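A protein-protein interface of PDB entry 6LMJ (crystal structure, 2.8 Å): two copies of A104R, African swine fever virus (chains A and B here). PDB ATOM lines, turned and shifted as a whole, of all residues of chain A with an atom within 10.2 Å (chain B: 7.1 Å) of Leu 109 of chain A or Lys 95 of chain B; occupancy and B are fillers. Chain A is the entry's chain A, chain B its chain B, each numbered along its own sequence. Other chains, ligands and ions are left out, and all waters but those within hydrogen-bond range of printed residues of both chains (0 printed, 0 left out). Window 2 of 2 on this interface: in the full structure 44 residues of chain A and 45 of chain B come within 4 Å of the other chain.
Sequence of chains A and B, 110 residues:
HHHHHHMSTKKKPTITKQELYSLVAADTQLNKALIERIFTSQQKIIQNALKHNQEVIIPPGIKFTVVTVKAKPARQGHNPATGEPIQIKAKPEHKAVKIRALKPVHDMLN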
ATOM      1  N   LEU A 102      -4.365 -21.758  11.164  1.00  0.00           N
ATOM      2  CA  LEU A 102      -4.472 -22.560  12.373  1.00  0.00           C
ATOM      3  C   LEU A 102      -3.226 -23.428  12.513  1.00  0.00           C
ATOM      4  O   LEU A 102      -2.581 -23.787  11.529  1.00  0.00           O
ATOM      5  CB  LEU A 102      -5.731 -23.428  12.345  1.00  0.00           C
ATOM      6  CG  LEU A 102      -7.105 -22.775  12.145  1.00  0.00           C
ATOM      7  CD1 LEU A 102      -8.192 -23.616  12.799  1.00  0.00           C
ATOM      8  CD2 LEU A 102      -7.154 -21.353  12.681  1.00  0.00           C
ATOM      9  N   LYS A 103      -2.895 -23.769  13.753  1.00  0.00           N
ATOM     10  CA  LYS A 103      -1.618 -24.412  14.049  1.00  0.00           C
ATOM     11  C   LYS A 103      -1.402 -25.777  13.385  1.00  0.00           C
ATOM     12  O   LYS A 103      -0.244 -26.164  13.181  1.00  0.00           O
ATOM     13  CB  LYS A 103      -1.437 -24.543  15.561  1.00  0.00           C
ATOM     14  CG  LYS A 103       0.026 -24.687  15.950  1.00  0.00           C
ATOM     15  CD  LYS A 103       0.243 -25.714  17.043  1.00  0.00           C
ATOM     16  CE  LYS A 103       1.390 -25.290  17.947  1.00  0.00           C
ATOM     17  NZ  LYS A 103       1.756 -26.357  18.915  1.00  0.00           N
ATOM     18  N   PRO A 104      -2.461 -26.559  13.039  1.00  0.00           N
ATOM     19  CA  PRO A 104      -2.222 -27.755  12.214  1.00  0.00           C
ATOM     20  C   PRO A 104      -1.441 -27.463  10.939  1.00  0.00           C
ATOM     21  O   PRO A 104      -0.846 -28.367  10.346  1.00  0.00           O
ATOM     22  CB  PRO A 104      -3.639 -28.244  11.897  1.00  0.00           C
ATOM     23  CG  PRO A 104      -4.408 -27.877  13.100  1.00  0.00           C
ATOM     24  CD  PRO A 104      -3.821 -26.581  13.612  1.00  0.00           C
ATOM     25  N   VAL A 105      -1.436 -26.199  10.518  1.00  0.00           N
ATOM     26  CA  VAL A 105      -0.683 -25.786   9.340  1.00  0.00           C
ATOM     27  C   VAL A 105       0.784 -25.513   9.666  1.00  0.00           C
ATOM     28  O   VAL A 105       1.663 -25.799   8.845  1.00  0.00           O
ATOM     29  CB  VAL A 105      -1.357 -24.556   8.706  1.00  0.00           C
ATOM     30  CG1 VAL A 105      -0.515 -23.997   7.573  1.00  0.00           C
ATOM     31  CG2 VAL A 105      -2.754 -24.910   8.219  1.00  0.00           C
ATOM     32  N   HIS A 106       1.073 -24.971  10.852  1.00  0.00           N
ATOM     33  CA  HIS A 106       2.462 -24.764  11.245  1.00  0.00           C
ATOM     34  C   HIS A 106       3.151 -26.081  11.574  1.00  0.00           C
ATOM     35  O   HIS A 106       4.379 -26.178  11.469  1.00  0.00           O
ATOM     36  CB  HIS A 106       2.540 -23.813  12.440  1.00  0.00           C
ATOM     37  CG  HIS A 106       1.961 -22.458  12.175  1.00  0.00           C
ATOM     38  ND1 HIS A 106       0.881 -21.962  12.873  1.00  0.00           N
ATOM     39  CD2 HIS A 106       2.312 -21.496  11.289  1.00  0.00           C
ATOM     40  CE1 HIS A 106       0.591 -20.752  12.429  1.00  0.00           C
ATOM     41  NE2 HIS A 106       1.444 -20.446  11.467  1.00  0.00           N
ATOM     42  N   ASP A 107       2.384 -27.095  11.974  1.00  0.00           N
ATOM     43  CA  ASP A 107       2.945 -28.411  12.253  1.00  0.00           C
ATOM     44  C   ASP A 107       3.435 -29.122  11.000  1.00  0.00           C
ATOM     45  O   ASP A 107       4.116 -30.145  11.117  1.00  0.00           O
ATOM     46  CB  ASP A 107       1.910 -29.282  12.965  1.00  0.00           C
ATOM     47  CG  ASP A 107       1.371 -28.635  14.224  1.00  0.00           C
ATOM     48  OD1 ASP A 107       1.901 -27.576  14.624  1.00  0.00           O
ATOM     49  OD2 ASP A 107       0.418 -29.184  14.815  1.00  0.00           O
ATOM     50  N   MET A 108       3.103 -28.612   9.810  1.00  0.00           N
ATOM     51  CA  MET A 108       3.593 -29.214   8.577  1.00  0.00           C
ATOM     52  C   MET A 108       5.109 -29.130   8.460  1.00  0.00           C
ATOM     53  O   MET A 108       5.702 -29.879   7.677  1.00  0.00           O
ATOM     54  CB  MET A 108       2.935 -28.546   7.368  1.00  0.00           C
ATOM     55  CG  MET A 108       1.458 -28.875   7.212  1.00  0.00           C
ATOM     56  SD  MET A 108       0.806 -28.442   5.587  1.00  0.00           S
ATOM     57  CE  MET A 108       0.862 -26.657   5.666  1.00  0.00           C
ATOM     58  N   LEU A 109       5.748 -28.239   9.220  1.00  0.00           N
ATOM     59  CA  LEU A 109       7.201 -28.138   9.267  1.00  0.00           C
ATOM     60  C   LEU A 109       7.795 -28.925  10.431  1.00  0.00           C
ATOM     61  O   LEU A 109       8.892 -28.607  10.903  1.00  0.00           O
ATOM     62  CB  LEU A 109       7.630 -26.673   9.342  1.00  0.00           C
ATOM     63  CG  LEU A 109       7.166 -25.763   8.203  1.00  0.00           C
ATOM     64  CD1 LEU A 109       7.930 -24.448   8.224  1.00  0.00           C
ATOM     65  CD2 LEU A 109       7.317 -26.454   6.855  1.00  0.00           C
ATOM     66  N   ASN A 110       7.086 -29.945  10.908  1.00  0.00           N
ATOM     67  CA  ASN A 110       7.577 -30.777  11.999  1.00  0.00           C
ATOM     68  C   ASN A 110       7.912 -32.179  11.501  1.00  0.00           C
ATOM     69  O   ASN A 110       7.629 -32.525  10.354  1.00  0.00           O
ATOM     70  CB  ASN A 110       6.546 -30.852  13.129  1.00  0.00           C
ATOM     71  CG  ASN A 110       6.251 -29.496  13.743  1.00  0.00           C
ATOM     72  OD1 ASN A 110       6.451 -28.459  13.113  1.00  0.00           O
ATOM     73  ND2 ASN A 110       5.772 -29.501  14.981  1.00  0.00           N
ATOM     74  N   ILE B  46       1.080 -30.302   0.140  1.00  0.00           N
ATOM     75  CA  ILE B  46       1.497 -29.022   0.710  1.00  0.00           C
ATOM     76  C   ILE B  46       2.689 -29.217   1.640  1.00  0.00           C
ATOM     77  O   ILE B  46       3.708 -28.526   1.524  1.00  0.00           O
ATOM     78  CB  ILE B  46       0.327 -28.335   1.443  1.00  0.00           C
ATOM     79  CG1 ILE B  46      -0.978 -28.401   0.642  1.00  0.00           C
ATOM     80  CG2 ILE B  46       0.683 -26.892   1.768  1.00  0.00           C
ATOM     81  CD1 ILE B  46      -0.863 -28.029  -0.821  1.00  0.00           C
ATOM     82  N   GLN B  47       2.575 -30.160   2.581  1.00  0.00           N
ATOM     83  CA  GLN B  47       3.623 -30.363   3.579  1.00  0.00           C
ATOM     84  C   GLN B  47       4.956 -30.715   2.926  1.00  0.00           C
ATOM     85  O   GLN B  47       5.992 -30.118   3.240  1.00  0.00           O
ATOM     86  CB  GLN B  47       3.198 -31.455   4.561  1.00  0.00           C
ATOM     87  CG  GLN B  47       4.275 -31.854   5.550  1.00  0.00           C
ATOM     88  CD  GLN B  47       3.761 -32.802   6.614  1.00  0.00           C
ATOM     89  OE1 GLN B  47       2.591 -32.749   6.995  1.00  0.00           O
ATOM     90  NE2 GLN B  47       4.634 -33.675   7.099  1.00  0.00           N
ATOM     91  N   ALA B  49       5.908 -30.067  -0.020  1.00  0.00           N
ATOM     92  CA  ALA B  49       6.402 -28.923  -0.781  1.00  0.00           C
ATOM     93  C   ALA B  49       7.088 -27.913   0.130  1.00  0.00           C
ATOM     94  O   ALA B  49       8.231 -27.512  -0.121  1.00  0.00           O
ATOM     95  CB  ALA B  49       5.254 -28.270  -1.549  1.00  0.00           C
ATOM     96  N   LEU B  50       6.400 -27.483   1.193  1.00  0.00           N
ATOM     97  CA  LEU B  50       7.002 -26.545   2.135  1.00  0.00           C
ATOM     98  C   LEU B  50       8.253 -27.123   2.783  1.00  0.00           C
ATOM     99  O   LEU B  50       9.197 -26.380   3.079  1.00  0.00           O
ATOM    100  CB  LEU B  50       5.987 -26.150   3.206  1.00  0.00           C
ATOM    101  CG  LEU B  50       4.682 -25.525   2.709  1.00  0.00           C
ATOM    102  CD1 LEU B  50       3.687 -25.419   3.847  1.00  0.00           C
ATOM    103  CD2 LEU B  50       4.939 -24.161   2.091  1.00  0.00           C
ATOM    104  N   LYS B  51       8.280 -28.438   3.013  1.00  0.00           N
ATOM    105  CA  LYS B  51       9.479 -29.068   3.554  1.00  0.00           C
ATOM    106  C   LYS B  51      10.648 -28.964   2.582  1.00  0.00           C
ATOM    107  O   LYS B  51      11.809 -28.960   3.006  1.00  0.00           O
ATOM    108  CB  LYS B  51       9.196 -30.532   3.892  1.00  0.00           C
ATOM    109  CG  LYS B  51       8.805 -30.772   5.340  1.00  0.00           C
ATOM    110  CD  LYS B  51       8.823 -32.255   5.675  1.00  0.00           C
ATOM    111  CE  LYS B  51       8.731 -32.486   7.174  1.00  0.00           C
ATOM    112  NZ  LYS B  51       7.415 -32.059   7.723  1.00  0.00           N
ATOM    113  N   HIS B  52      10.362 -28.880   1.283  1.00  0.00           N
ATOM    114  CA  HIS B  52      11.383 -28.685   0.263  1.00  0.00           C
ATOM    115  C   HIS B  52      11.517 -27.221  -0.144  1.00  0.00           C
ATOM    116  O   HIS B  52      12.059 -26.929  -1.217  1.00  0.00           O
ATOM    117  CB  HIS B  52      11.083 -29.558  -0.956  1.00  0.00           C
ATOM    118  CG  HIS B  52      11.365 -31.012  -0.739  1.00  0.00           C
ATOM    119  ND1 HIS B  52      11.000 -31.678   0.411  1.00  0.00           N
ATOM    120  CD2 HIS B  52      11.980 -31.929  -1.524  1.00  0.00           C
ATOM    121  CE1 HIS B  52      11.376 -32.942   0.325  1.00  0.00           C
ATOM    122  NE2 HIS B  52      11.973 -33.120  -0.840  1.00  0.00           N
ATOM    123  N   ASN B  53      11.022 -26.303   0.689  1.00  0.00           N
ATOM    124  CA  ASN B  53      11.185 -24.862   0.491  1.00  0.00           C
ATOM    125  C   ASN B  53      10.550 -24.390  -0.815  1.00  0.00           C
ATOM    126  O   ASN B  53      11.095 -23.539  -1.522  1.00  0.00           O
ATOM    127  CB  ASN B  53      12.660 -24.460   0.557  1.00  0.00           C
ATOM    128  CG  ASN B  53      13.199 -24.462   1.972  1.00  0.00           C
ATOM    129  OD1 ASN B  53      13.463 -25.520   2.546  1.00  0.00           O
ATOM    130  ND2 ASN B  53      13.358 -23.276   2.547  1.00  0.00           N
ATOM    131  N   THR B  65       3.645 -20.352   2.112  1.00  0.00           N
ATOM    132  CA  THR B  65       5.006 -19.834   2.084  1.00  0.00           C
ATOM    133  C   THR B  65       5.717 -20.174   3.385  1.00  0.00           C
ATOM    134  O   THR B  65       5.166 -19.966   4.470  1.00  0.00           O
ATOM    135  CB  THR B  65       5.014 -18.315   1.872  1.00  0.00           C
ATOM    136  OG1 THR B  65       4.120 -17.966   0.805  1.00  0.00           O
ATOM    137  CG2 THR B  65       6.413 -17.831   1.531  1.00  0.00           C
ATOM    138  N   VAL B  66       6.936 -20.694   3.267  1.00  0.00           N
ATOM    139  CA  VAL B  66       7.834 -20.840   4.408  1.00  0.00           C
ATOM    140  C   VAL B  66       8.496 -19.495   4.671  1.00  0.00           C
ATOM    141  O   VAL B  66       8.827 -18.761   3.732  1.00  0.00           O
ATOM    142  CB  VAL B  66       8.876 -21.940   4.129  1.00  0.00           C
ATOM    143  CG1 VAL B  66       9.971 -21.938   5.186  1.00  0.00           C
ATOM    144  CG2 VAL B  66       8.207 -23.304   4.045  1.00  0.00           C
ATOM    145  N   VAL B  67       8.686 -19.147   5.944  1.00  0.00           N
ATOM    146  CA  VAL B  67       9.270 -17.857   6.298  1.00  0.00           C
ATOM    147  C   VAL B  67       9.962 -17.972   7.649  1.00  0.00           C
ATOM    148  O   VAL B  67       9.630 -18.832   8.466  1.00  0.00           O
ATOM    149  CB  VAL B  67       8.198 -16.737   6.299  1.00  0.00           C
ATOM    150  CG1 VAL B  67       7.429 -16.724   7.613  1.00  0.00           C
ATOM    151  CG2 VAL B  67       8.847 -15.386   6.036  1.00  0.00           C
ATOM    152  N   THR B  68      10.931 -17.091   7.881  1.00  0.00           N
ATOM    153  CA  THR B  68      11.719 -17.055   9.105  1.00  0.00           C
ATOM    154  C   THR B  68      11.178 -15.969  10.026  1.00  0.00           C
ATOM    155  O   THR B  68      10.936 -14.840   9.587  1.00  0.00           O
ATOM    156  CB  THR B  68      13.193 -16.780   8.792  1.00  0.00           C
ATOM    157  OG1 THR B  68      13.608 -17.586   7.683  1.00  0.00           O
ATOM    158  CG2 THR B  68      14.065 -17.085   9.998  1.00  0.00           C
ATOM    159  N   VAL B  69      10.979 -16.308  11.296  1.00  0.00           N
ATOM    160  CA  VAL B  69      10.527 -15.345  12.293  1.00  0.00           C
ATOM    161  C   VAL B  69      11.659 -15.146  13.291  1.00  0.00           C
ATOM    162  O   VAL B  69      12.154 -16.110  13.890  1.00  0.00           O
ATOM    163  CB  VAL B  69       9.212 -15.789  12.959  1.00  0.00           C
ATOM    164  CG1 VAL B  69       9.371 -17.093  13.693  1.00  0.00           C
ATOM    165  CG2 VAL B  69       8.681 -14.694  13.881  1.00  0.00           C
ATOM    166  N   PRO B  92      12.613 -18.395  20.621  1.00  0.00           N
ATOM    167  CA  PRO B  92      13.762 -18.348  19.708  1.00  0.00           C
ATOM    168  C   PRO B  92      13.349 -18.203  18.253  1.00  0.00           C
ATOM    169  O   PRO B  92      12.157 -18.175  17.931  1.00  0.00           O
ATOM    170  CB  PRO B  92      14.457 -19.692  19.960  1.00  0.00           C
ATOM    171  CG  PRO B  92      13.353 -20.596  20.411  1.00  0.00           C
ATOM    172  CD  PRO B  92      12.415 -19.733  21.206  1.00  0.00           C
ATOM    173  N   GLU B  93      14.334 -18.102  17.367  1.00  0.00           N
ATOM    174  CA  GLU B  93      14.061 -18.084  15.941  1.00  0.00           C
ATOM    175  C   GLU B  93      13.512 -19.435  15.494  1.00  0.00           C
ATOM    176  O   GLU B  93      13.874 -20.486  16.031  1.00  0.00           O
ATOM    177  CB  GLU B  93      15.335 -17.747  15.166  1.00  0.00           C
ATOM    178  CG  GLU B  93      15.116 -17.217  13.760  1.00  0.00           C
ATOM    179  CD  GLU B  93      16.290 -16.393  13.261  1.00  0.00           C
ATOM    180  OE1 GLU B  93      17.054 -15.872  14.102  1.00  0.00           O
ATOM    181  OE2 GLU B  93      16.449 -16.269  12.028  1.00  0.00           O
ATOM    182  N   HIS B  94      12.624 -19.395  14.505  1.00  0.00           N
ATOM    183  CA  HIS B  94      12.041 -20.605  13.938  1.00  0.00           C
ATOM    184  C   HIS B  94      11.413 -20.253  12.597  1.00  0.00           C
ATOM    185  O   HIS B  94      11.287 -19.083  12.235  1.00  0.00           O
ATOM    186  CB  HIS B  94      11.013 -21.245  14.882  1.00  0.00           C
ATOM    187  CG  HIS B  94       9.914 -20.324  15.320  1.00  0.00           C
ATOM    188  ND1 HIS B  94       8.637 -20.394  14.805  1.00  0.00           N
ATOM    189  CD2 HIS B  94       9.895 -19.327  16.237  1.00  0.00           C
ATOM    190  CE1 HIS B  94       7.880 -19.480  15.385  1.00  0.00           C
ATOM    191  NE2 HIS B  94       8.618 -18.819  16.259  1.00  0.00           N
ATOM    192  N   LYS B  95      11.056 -21.288  11.849  1.00  0.00           N
ATOM    193  CA  LYS B  95      10.317 -21.127  10.608  1.00  0.00           C
ATOM    194  C   LYS B  95       8.820 -21.262  10.866  1.00  0.00           C
ATOM    195  O   LYS B  95       8.387 -21.982  11.769  1.00  0.00           O
ATOM    196  CB  LYS B  95      10.766 -22.154   9.566  1.00  0.00           C
ATOM    197  CG  LYS B  95      12.265 -22.403   9.545  1.00  0.00           C
ATOM    198  CD  LYS B  95      12.915 -21.720   8.345  1.00  0.00           C
ATOM    199  CE  LYS B  95      14.114 -22.503   7.841  1.00  0.00           C
ATOM    200  NZ  LYS B  95      14.224 -22.442   6.360  1.00  0.00           N
ATOM    201  N   ALA B  96       8.030 -20.554  10.065  1.00  0.00           N
ATOM    202  CA  ALA B  96       6.582 -20.550  10.211  1.00  0.00           C
ATOM    203  C   ALA B  96       5.950 -20.499   8.830  1.00  0.00           C
ATOM    204  O   ALA B  96       6.475 -19.845   7.926  1.00  0.00           O
ATOM    205  CB  ALA B  96       6.107 -19.366  11.060  1.00  0.00           C
ATOM    206  N   VAL B  97       4.834 -21.203   8.672  1.00  0.00           N
ATOM    207  CA  VAL B  97       4.131 -21.253   7.395  1.00  0.00           C
ATOM    208  C   VAL B  97       3.243 -20.016   7.298  1.00  0.00           C
ATOM    209  O   VAL B  97       2.293 -19.863   8.068  1.00  0.00           O
ATOM    210  CB  VAL B  97       3.310 -22.539   7.255  1.00  0.00           C
ATOM    211  CG1 VAL B  97       2.563 -22.549   5.932  1.00  0.00           C
ATOM    212  CG2 VAL B  97       4.213 -23.759   7.374  1.00  0.00           C
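Pro 104 of chain A touches none of the printed residues of chain B.
Of the printed residues of chain B, His 106 of chain A touches Val 97 (3.6 Å).
Leu 109 of chain A touches three residues of chain B.
Printed residues of chain A within 4 Å of Ile 46 of chain B: Met 108.
No residue of chain A comes within 4 Å of His 94 of chain B.
Lys 95 of chain B touches one residue of chain A.
No residue of chain A comes within 4 Å of Ala 96 of chain B.
Printed residues of chain A within 4 Å of Val 97 of chain B: Val 105, His 106 and Leu 109.
The nearest residue of chain B that does not touch Leu 109 of chain A is Lys 51 of chain B (4.2 Å).
The nearest residue of chain A that does not touch Lys 95 of chain B is His 106 of chain A (5.8 Å).
The nearest printed residue of chain A that does not touch Gln 47 of chain B is Asn 110 of chain A (4.6 Å).
No position is printed for both chains.
Among the printed residues, merely in contact across the chains: Met 108 of chain A with Gln 47 of chain B (3.2 Å), His 106 of chain A with Val 97 of chain B (3.6 Å), Met 108 of chain A with Leu 50 of chain B (3.6 Å), Val 105 of chain A with Val 97 of chain B (3.6 Å), Leu 109 of chain A with Val 97 of chain B (3.7 Å), Leu 109 of chain A with Lys 95 of chain B (3.9 Å), Leu 109 of chain A with Leu 50 of chain B (3.9 Å) and Met 108 of chain A with Ile 46 of chain B (3.9 Å).
The backbone carbonyl oxygen (O) of Met 108 of chain A lies within hydrogen-bond range of the side-chain amino group (NZ) of Lys 51 of chain B, at 2.8 Å.
The backbone carbonyl oxygen of Asn 110 of chain A is in hydrogen-bond range of the side-chain amino group of Lys 51 of chain B, 2.7 Å away.
O of His 106 of chain A sits close to OD1 of Asn 110 of chain A (3.5 Å).
The side-chain amide nitrogen of Gln 47 of chain B lies close to the side-chain amino group of Lys 51 of chain B, 3.3 Å away.
Of the 18 printed residues of chain B, 6 touch a printed residue of chain A.
Hydrophobic or aromatic side chains of chain B that line the printed part of chain A: Ile 46, Leu 50 and Val 97.
Among the printed residues, 10 pairs touch across the chains.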
